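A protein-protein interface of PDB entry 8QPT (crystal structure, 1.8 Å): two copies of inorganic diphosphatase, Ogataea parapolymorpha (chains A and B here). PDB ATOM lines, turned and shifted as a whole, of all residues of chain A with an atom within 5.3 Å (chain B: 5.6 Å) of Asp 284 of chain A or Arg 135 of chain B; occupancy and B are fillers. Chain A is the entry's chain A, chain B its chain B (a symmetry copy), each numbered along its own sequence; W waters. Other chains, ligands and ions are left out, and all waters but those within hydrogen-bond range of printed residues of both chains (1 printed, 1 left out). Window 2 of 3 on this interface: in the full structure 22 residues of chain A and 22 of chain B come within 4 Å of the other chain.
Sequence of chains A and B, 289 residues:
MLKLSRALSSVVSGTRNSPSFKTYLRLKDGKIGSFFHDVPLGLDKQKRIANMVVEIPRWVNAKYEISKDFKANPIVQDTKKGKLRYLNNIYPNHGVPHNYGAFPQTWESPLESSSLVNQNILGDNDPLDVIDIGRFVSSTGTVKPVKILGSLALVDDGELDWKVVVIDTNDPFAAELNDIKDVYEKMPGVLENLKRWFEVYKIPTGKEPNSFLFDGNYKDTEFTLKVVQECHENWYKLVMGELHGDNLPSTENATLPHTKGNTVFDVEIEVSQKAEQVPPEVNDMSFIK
The guanidinium group (NH2) of Arg 58 of chain B is in hydrogen-bond range of the backbone carbonyl oxygen (O) of Asn 283 of chain A (2.9 Å).
SD of Met 285 of chain A lies close to NE of Arg 58 of chain B, at 3.8 Å.
NH1 of Arg 58 of chain B lies within hydrogen-bond range of O of Gly 134 of chain B, at 3.0 Å.
The backbone NH (N) of Ser 286 of chain A sits at hydrogen-bond distance from the backbone carbonyl oxygen (O) of Asn 89 of chain A, at 2.8 Å.
The backbone carbonyl oxygen (O) of Asp 284 of chain A sits at hydrogen-bond distance from the side-chain amide nitrogen (ND2) of Asn 89 of chain A, 2.9 Å away.
NH1 of Arg 58 of chain B lies within hydrogen-bond range of O of Phe 136 of chain B (3.2 Å).
The side-chain carboxylate (OD1) of Asp 171 of chain B is in salt-bridge range of the guanidinium group (NH2) of Arg 135 of chain B (2.9 Å).
ND2 of Asn 89 of chain A lies within hydrogen-bond range of O of Val 282 of chain A (2.8 Å).
Among the printed residues, merely in contact across the chains: Asn 89 of chain A with Trp 59 of chain B, Asn 283 of chain A with Trp 59 of chain B, Asn 283 of chain A with Val 137 of chain B, Asp 284 of chain A with Arg 135 of chain B, Met 285 of chain A with Trp 59 of chain B, Met 285 of chain A with Ile 133 of chain B and Met 285 of chain A with Gly 134 of chain B.
Asp 284 of chain A touches just one residue of chain B: Arg 135 (3.9 Å).
Ser 286 of chain A touches none of the printed residues of chain B.
Of the printed residues of chain A, Ile 133 of chain B touches Met 285 (3.9 Å).
Printed residues of chain A within 4 Å of Gly 134 of chain B: Met 285 (3.6 Å).
Arg 135 of chain B touches just one residue of chain A: Asp 284 (3.9 Å).
Asp 171 of chain B touches none of the printed residues of chain A.
The nearest residue of chain B that does not touch Asp 284 of chain A is Arg 58 of chain B (4.7 Å).
The nearest residue of chain A that does not touch Arg 135 of chain B is Asn 283 of chain A (4.3 Å).
Of the 8 printed residues of chain A, 4 touch a printed residue of chain B.
Along chain A the printed residues that touch a printed residue of chain B span positions 89 to 285.
Of the 11 printed residues of chain B, 6 touch a printed residue of chain A.
Hydrophobic or aromatic side chains of chain B within 4 Å of the printed part of chain A: Trp 59 and Val 137.
No position is printed for both chains.
Of the 9 pairs that touch across the chains among the printed residues, none has its exchanged pair printed and touching as well.
Water W1 lies within hydrogen-bond range of NE1 of Trp 59 of chain B (3.0 Å) and SD of Met 285 of chain A (3.8 Å).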
ATOM      1  N   ASN A  89      -9.720  15.558   3.524  1.00  0.00           N
ATOM      2  CA  ASN A  89      -8.916  15.277   4.745  1.00  0.00           C
ATOM      3  C   ASN A  89      -9.738  14.295   5.579  1.00  0.00           C
ATOM      4  O   ASN A  89     -10.641  14.720   6.301  1.00  0.00           O
ATOM      5  CB  ASN A  89      -8.566  16.569   5.478  1.00  0.00           C
ATOM      6  CG  ASN A  89      -7.832  17.529   4.571  1.00  0.00           C
ATOM      7  OD1 ASN A  89      -6.783  17.203   4.005  1.00  0.00           O
ATOM      8  ND2 ASN A  89      -8.407  18.666   4.263  1.00  0.00           N
ATOM      9  N   PRO A 280     -10.081  27.701  -0.095  1.00  0.00           N
ATOM     10  CA  PRO A 280     -10.071  27.464   1.358  1.00  0.00           C
ATOM     11  C   PRO A 280     -10.828  26.257   1.909  1.00  0.00           C
ATOM     12  O   PRO A 280     -10.370  25.645   2.876  1.00  0.00           O
ATOM     13  CB  PRO A 280     -10.662  28.763   1.982  1.00  0.00           C
ATOM     14  CG  PRO A 280     -11.226  29.568   0.780  1.00  0.00           C
ATOM     15  CD  PRO A 280     -10.543  29.059  -0.481  1.00  0.00           C
ATOM     16  N   GLU A 281     -11.930  25.853   1.273  1.00  0.00           N
ATOM     17  CA  GLU A 281     -12.734  24.671   1.678  1.00  0.00           C
ATOM     18  C   GLU A 281     -11.889  23.371   1.536  1.00  0.00           C
ATOM     19  O   GLU A 281     -12.232  22.325   2.112  1.00  0.00           O
ATOM     20  CB  GLU A 281     -13.977  24.478   0.813  1.00  0.00           C
ATOM     21  CG  GLU A 281     -14.510  25.752   0.224  1.00  0.00           C
ATOM     22  CD  GLU A 281     -13.759  26.187  -1.018  1.00  0.00           C
ATOM     23  OE1 GLU A 281     -13.008  27.133  -0.848  1.00  0.00           O
ATOM     24  OE2 GLU A 281     -13.838  25.497  -2.107  1.00  0.00           O
ATOM     25  N   VAL A 282     -10.803  23.399   0.763  1.00  0.00           N
ATOM     26  CA  VAL A 282      -9.901  22.186   0.654  1.00  0.00           C
ATOM     27  C   VAL A 282      -9.331  21.845   2.046  1.00  0.00           C
ATOM     28  O   VAL A 282      -9.102  20.640   2.331  1.00  0.00           O
ATOM     29  CB  VAL A 282      -8.815  22.402  -0.412  1.00  0.00           C
ATOM     30  CG1 VAL A 282      -7.782  21.261  -0.416  1.00  0.00           C
ATOM     31  CG2 VAL A 282      -9.421  22.451  -1.809  1.00  0.00           C
ATOM     32  N   ASN A 283      -9.189  22.823   2.936  1.00  0.00           N
ATOM     33  CA  ASN A 283      -8.608  22.595   4.263  1.00  0.00           C
ATOM     34  C   ASN A 283      -9.644  22.047   5.247  1.00  0.00           C
ATOM     35  O   ASN A 283      -9.235  21.636   6.325  1.00  0.00           O
ATOM     36  CB  ASN A 283      -7.914  23.810   4.828  1.00  0.00           C
ATOM     37  CG  ASN A 283      -6.675  24.133   4.038  1.00  0.00           C
ATOM     38  OD1 ASN A 283      -5.944  23.267   3.582  1.00  0.00           O
ATOM     39  ND2 ASN A 283      -6.454  25.404   3.868  1.00  0.00           N
ATOM     40  N   ASP A 284     -10.923  21.946   4.911  1.00  0.00           N
ATOM     41  CA  ASP A 284     -11.920  21.389   5.850  1.00  0.00           C
ATOM     42  C   ASP A 284     -11.604  19.935   6.106  1.00  0.00           C
ATOM     43  O   ASP A 284     -11.115  19.235   5.215  1.00  0.00           O
ATOM     44  CB  ASP A 284     -13.405  21.541   5.428  1.00  0.00           C
ATOM     45  CG  ASP A 284     -13.878  22.958   5.073  1.00  0.00           C
ATOM     46  OD1 ASP A 284     -13.157  24.024   5.330  1.00  0.00           O
ATOM     47  OD2 ASP A 284     -14.936  23.005   4.423  1.00  0.00           O
ATOM     48  N   MET A 285     -11.897  19.498   7.329  1.00  0.00           N
ATOM     49  CA  MET A 285     -11.710  18.113   7.755  1.00  0.00           C
ATOM     50  C   MET A 285     -13.025  17.341   7.601  1.00  0.00           C
ATOM     51  O   MET A 285     -14.088  17.962   7.916  1.00  0.00           O
ATOM     52  CB  MET A 285     -11.259  18.096   9.205  1.00  0.00           C
ATOM     53  CG  MET A 285      -9.774  18.717   9.328  1.00  0.00           C
ATOM     54  SD  MET A 285      -9.243  18.936  11.023  1.00  0.00           S
ATOM     55  CE  MET A 285     -10.165  20.409  11.432  1.00  0.00           C
ATOM     56  N   SER A 286     -12.909  16.075   7.298  1.00  0.00           N
ATOM     57  CA  SER A 286     -14.053  15.101   7.242  1.00  0.00           C
ATOM     58  C   SER A 286     -13.961  14.130   8.393  1.00  0.00           C
ATOM     59  O   SER A 286     -12.918  13.485   8.573  1.00  0.00           O
ATOM     60  CB  SER A 286     -14.077  14.382   5.914  1.00  0.00           C
ATOM     61  OG  SER A 286     -14.095  15.298   4.826  1.00  0.00           O
ATOM     62  N   ARG B  58      -3.070  24.799  12.296  1.00  0.00           N
ATOM     63  CA  ARG B  58      -3.221  23.390  11.977  1.00  0.00           C
ATOM     64  C   ARG B  58      -2.252  22.971  10.835  1.00  0.00           C
ATOM     65  O   ARG B  58      -2.059  23.704   9.818  1.00  0.00           O
ATOM     66  CB  ARG B  58      -4.691  23.097  11.664  1.00  0.00           C
ATOM     67  CG  ARG B  58      -4.897  21.633  11.381  1.00  0.00           C
ATOM     68  CD  ARG B  58      -6.384  21.281  11.204  1.00  0.00           C
ATOM     69  NE  ARG B  58      -7.002  21.796   9.965  1.00  0.00           N
ATOM     70  CZ  ARG B  58      -7.947  22.749   9.904  1.00  0.00           C
ATOM     71  NH1 ARG B  58      -8.258  23.508  10.953  1.00  0.00           N
ATOM     72  NH2 ARG B  58      -8.475  23.041   8.730  1.00  0.00           N
ATOM     73  N   TRP B  59      -1.614  21.833  11.041  1.00  0.00           N
ATOM     74  CA  TRP B  59      -0.780  21.043  10.110  1.00  0.00           C
ATOM     75  C   TRP B  59       0.576  21.738   9.993  1.00  0.00           C
ATOM     76  O   TRP B  59       1.307  21.338   9.055  1.00  0.00           O
ATOM     77  CB  TRP B  59      -1.431  20.814   8.752  1.00  0.00           C
ATOM     78  CG  TRP B  59      -2.712  20.052   8.897  1.00  0.00           C
ATOM     79  CD1 TRP B  59      -2.922  18.956   9.690  1.00  0.00           C
ATOM     80  CD2 TRP B  59      -3.923  20.241   8.138  1.00  0.00           C
ATOM     81  NE1 TRP B  59      -4.207  18.502   9.543  1.00  0.00           N
ATOM     82  CE2 TRP B  59      -4.831  19.257   8.578  1.00  0.00           C
ATOM     83  CE3 TRP B  59      -4.321  21.159   7.154  1.00  0.00           C
ATOM     84  CZ2 TRP B  59      -6.114  19.164   8.056  1.00  0.00           C
ATOM     85  CZ3 TRP B  59      -5.612  21.083   6.661  1.00  0.00           C
ATOM     86  CH2 TRP B  59      -6.490  20.096   7.116  1.00  0.00           C
ATOM     87  N   ILE B 133     -10.660  23.417  17.351  1.00  0.00           N
ATOM     88  CA  ILE B 133     -10.967  22.254  16.478  1.00  0.00           C
ATOM     89  C   ILE B 133     -11.808  22.695  15.279  1.00  0.00           C
ATOM     90  O   ILE B 133     -12.236  21.804  14.487  1.00  0.00           O
ATOM     91  CB  ILE B 133     -11.668  21.158  17.305  1.00  0.00           C
ATOM     92  CG1 ILE B 133     -13.002  21.650  17.848  1.00  0.00           C
ATOM     93  CG2 ILE B 133     -10.755  20.615  18.409  1.00  0.00           C
ATOM     94  CD1 ILE B 133     -13.864  20.522  18.458  1.00  0.00           C
ATOM     95  N   GLY B 134     -11.923  23.981  15.007  1.00  0.00           N
ATOM     96  CA  GLY B 134     -12.741  24.466  13.870  1.00  0.00           C
ATOM     97  C   GLY B 134     -12.094  24.344  12.505  1.00  0.00           C
ATOM     98  O   GLY B 134     -10.916  23.840  12.409  1.00  0.00           O
ATOM     99  N   ARG B 135     -12.827  24.699  11.441  1.00  0.00           N
ATOM    100  CA  ARG B 135     -12.446  24.335  10.072  1.00  0.00           C
ATOM    101  C   ARG B 135     -11.344  25.278   9.598  1.00  0.00           C
ATOM    102  O   ARG B 135     -10.634  24.916   8.670  1.00  0.00           O
ATOM    103  CB  ARG B 135     -13.705  24.405   9.181  1.00  0.00           C
ATOM    104  CG  ARG B 135     -14.157  25.817   8.866  1.00  0.00           C
ATOM    105  CD  ARG B 135     -15.444  25.668   8.030  1.00  0.00           C
ATOM    106  NE  ARG B 135     -16.376  25.008   8.911  1.00  0.00           N
ATOM    107  CZ  ARG B 135     -17.559  24.475   8.549  1.00  0.00           C
ATOM    108  NH1 ARG B 135     -18.001  24.608   7.295  1.00  0.00           N
ATOM    109  NH2 ARG B 135     -18.296  23.850   9.469  1.00  0.00           N
ATOM    110  N   PHE B 136     -11.263  26.483  10.135  1.00  0.00           N
ATOM    111  CA  PHE B 136     -10.368  27.505   9.604  1.00  0.00           C
ATOM    112  C   PHE B 136      -8.948  27.121  10.046  1.00  0.00           C
ATOM    113  O   PHE B 136      -8.740  26.693  11.209  1.00  0.00           O
ATOM    114  CB  PHE B 136     -10.694  28.928  10.025  1.00  0.00           C
ATOM    115  CG  PHE B 136     -12.112  29.311   9.763  1.00  0.00           C
ATOM    116  CD1 PHE B 136     -12.532  29.458   8.446  1.00  0.00           C
ATOM    117  CD2 PHE B 136     -13.047  29.381  10.804  1.00  0.00           C
ATOM    118  CE1 PHE B 136     -13.881  29.695   8.177  1.00  0.00           C
ATOM    119  CE2 PHE B 136     -14.377  29.698  10.527  1.00  0.00           C
ATOM    120  CZ  PHE B 136     -14.783  29.815   9.217  1.00  0.00           C
ATOM    121  N   VAL B 137      -8.012  27.371   9.120  1.00  0.00           N
ATOM    122  CA  VAL B 137      -6.564  27.311   9.538  1.00  0.00           C
ATOM    123  C   VAL B 137      -6.187  28.732   9.896  1.00  0.00           C
ATOM    124  O   VAL B 137      -6.368  29.636   9.018  1.00  0.00           O
ATOM    125  CB  VAL B 137      -5.703  26.742   8.402  1.00  0.00           C
ATOM    126  CG1 VAL B 137      -4.217  26.752   8.831  1.00  0.00           C
ATOM    127  CG2 VAL B 137      -6.124  25.336   7.983  1.00  0.00           C
ATOM    128  N   ILE B 167     -13.774  25.933  19.875  1.00  0.00           N
ATOM    129  CA  ILE B 167     -14.016  26.111  18.446  1.00  0.00           C
ATOM    130  C   ILE B 167     -14.189  27.601  18.148  1.00  0.00           C
ATOM    131  O   ILE B 167     -14.957  28.291  18.880  1.00  0.00           O
ATOM    132  CB  ILE B 167     -15.198  25.248  17.950  1.00  0.00           C
ATOM    133  CG1 ILE B 167     -15.281  25.326  16.437  1.00  0.00           C
ATOM    134  CG2 ILE B 167     -16.524  25.653  18.605  1.00  0.00           C
ATOM    135  CD1 ILE B 167     -16.205  24.272  15.830  1.00  0.00           C
ATOM    136  N   ASP B 171     -17.077  29.384  13.063  1.00  0.00           N
ATOM    137  CA  ASP B 171     -17.297  28.094  12.413  1.00  0.00           C
ATOM    138  C   ASP B 171     -18.828  27.866  12.440  1.00  0.00           C
ATOM    139  O   ASP B 171     -19.355  27.747  13.528  1.00  0.00           O
ATOM    140  CB  ASP B 171     -16.615  26.958  13.146  1.00  0.00           C
ATOM    141  CG  ASP B 171     -16.630  25.682  12.330  1.00  0.00           C
ATOM    142  OD1 ASP B 171     -17.766  25.289  11.885  1.00  0.00           O
ATOM    143  OD2 ASP B 171     -15.544  25.083  12.120  1.00  0.00           O
ATOM    144  N   PRO B 172     -19.538  27.773  11.300  1.00  0.00           N
ATOM    145  CA  PRO B 172     -21.000  27.515  11.333  1.00  0.00           C
ATOM    146  C   PRO B 172     -21.388  26.314  12.207  1.00  0.00           C
ATOM    147  O   PRO B 172     -22.439  26.317  12.778  1.00  0.00           O
ATOM    148  CB  PRO B 172     -21.321  27.256   9.871  1.00  0.00           C
ATOM    149  CG  PRO B 172     -20.274  28.079   9.143  1.00  0.00           C
ATOM    150  CD  PRO B 172     -18.998  27.871   9.938  1.00  0.00           C
ATOM    151  N   PHE B 173     -20.494  25.357  12.430  1.00  0.00           N
ATOM    152  CA  PHE B 173     -20.779  24.178  13.271  1.00  0.00           C
ATOM    153  C   PHE B 173     -20.752  24.501  14.763  1.00  0.00           C
ATOM    154  O   PHE B 173     -21.244  23.740  15.584  1.00  0.00           O
ATOM    155  CB  PHE B 173     -19.895  23.015  12.812  1.00  0.00           C
ATOM    156  CG  PHE B 173     -20.449  21.672  13.193  1.00  0.00           C
ATOM    157  CD1 PHE B 173     -19.800  20.860  14.117  1.00  0.00           C
ATOM    158  CD2 PHE B 173     -21.673  21.253  12.670  1.00  0.00           C
ATOM    159  CE1 PHE B 173     -20.357  19.647  14.500  1.00  0.00           C
ATOM    160  CE2 PHE B 173     -22.207  20.026  13.032  1.00  0.00           C
ATOM    161  CZ  PHE B 173     -21.559  19.234  13.950  1.00  0.00           C
HETATM  162  O   HOH W   1      -5.984  17.078  11.512  1.00  0.00           O
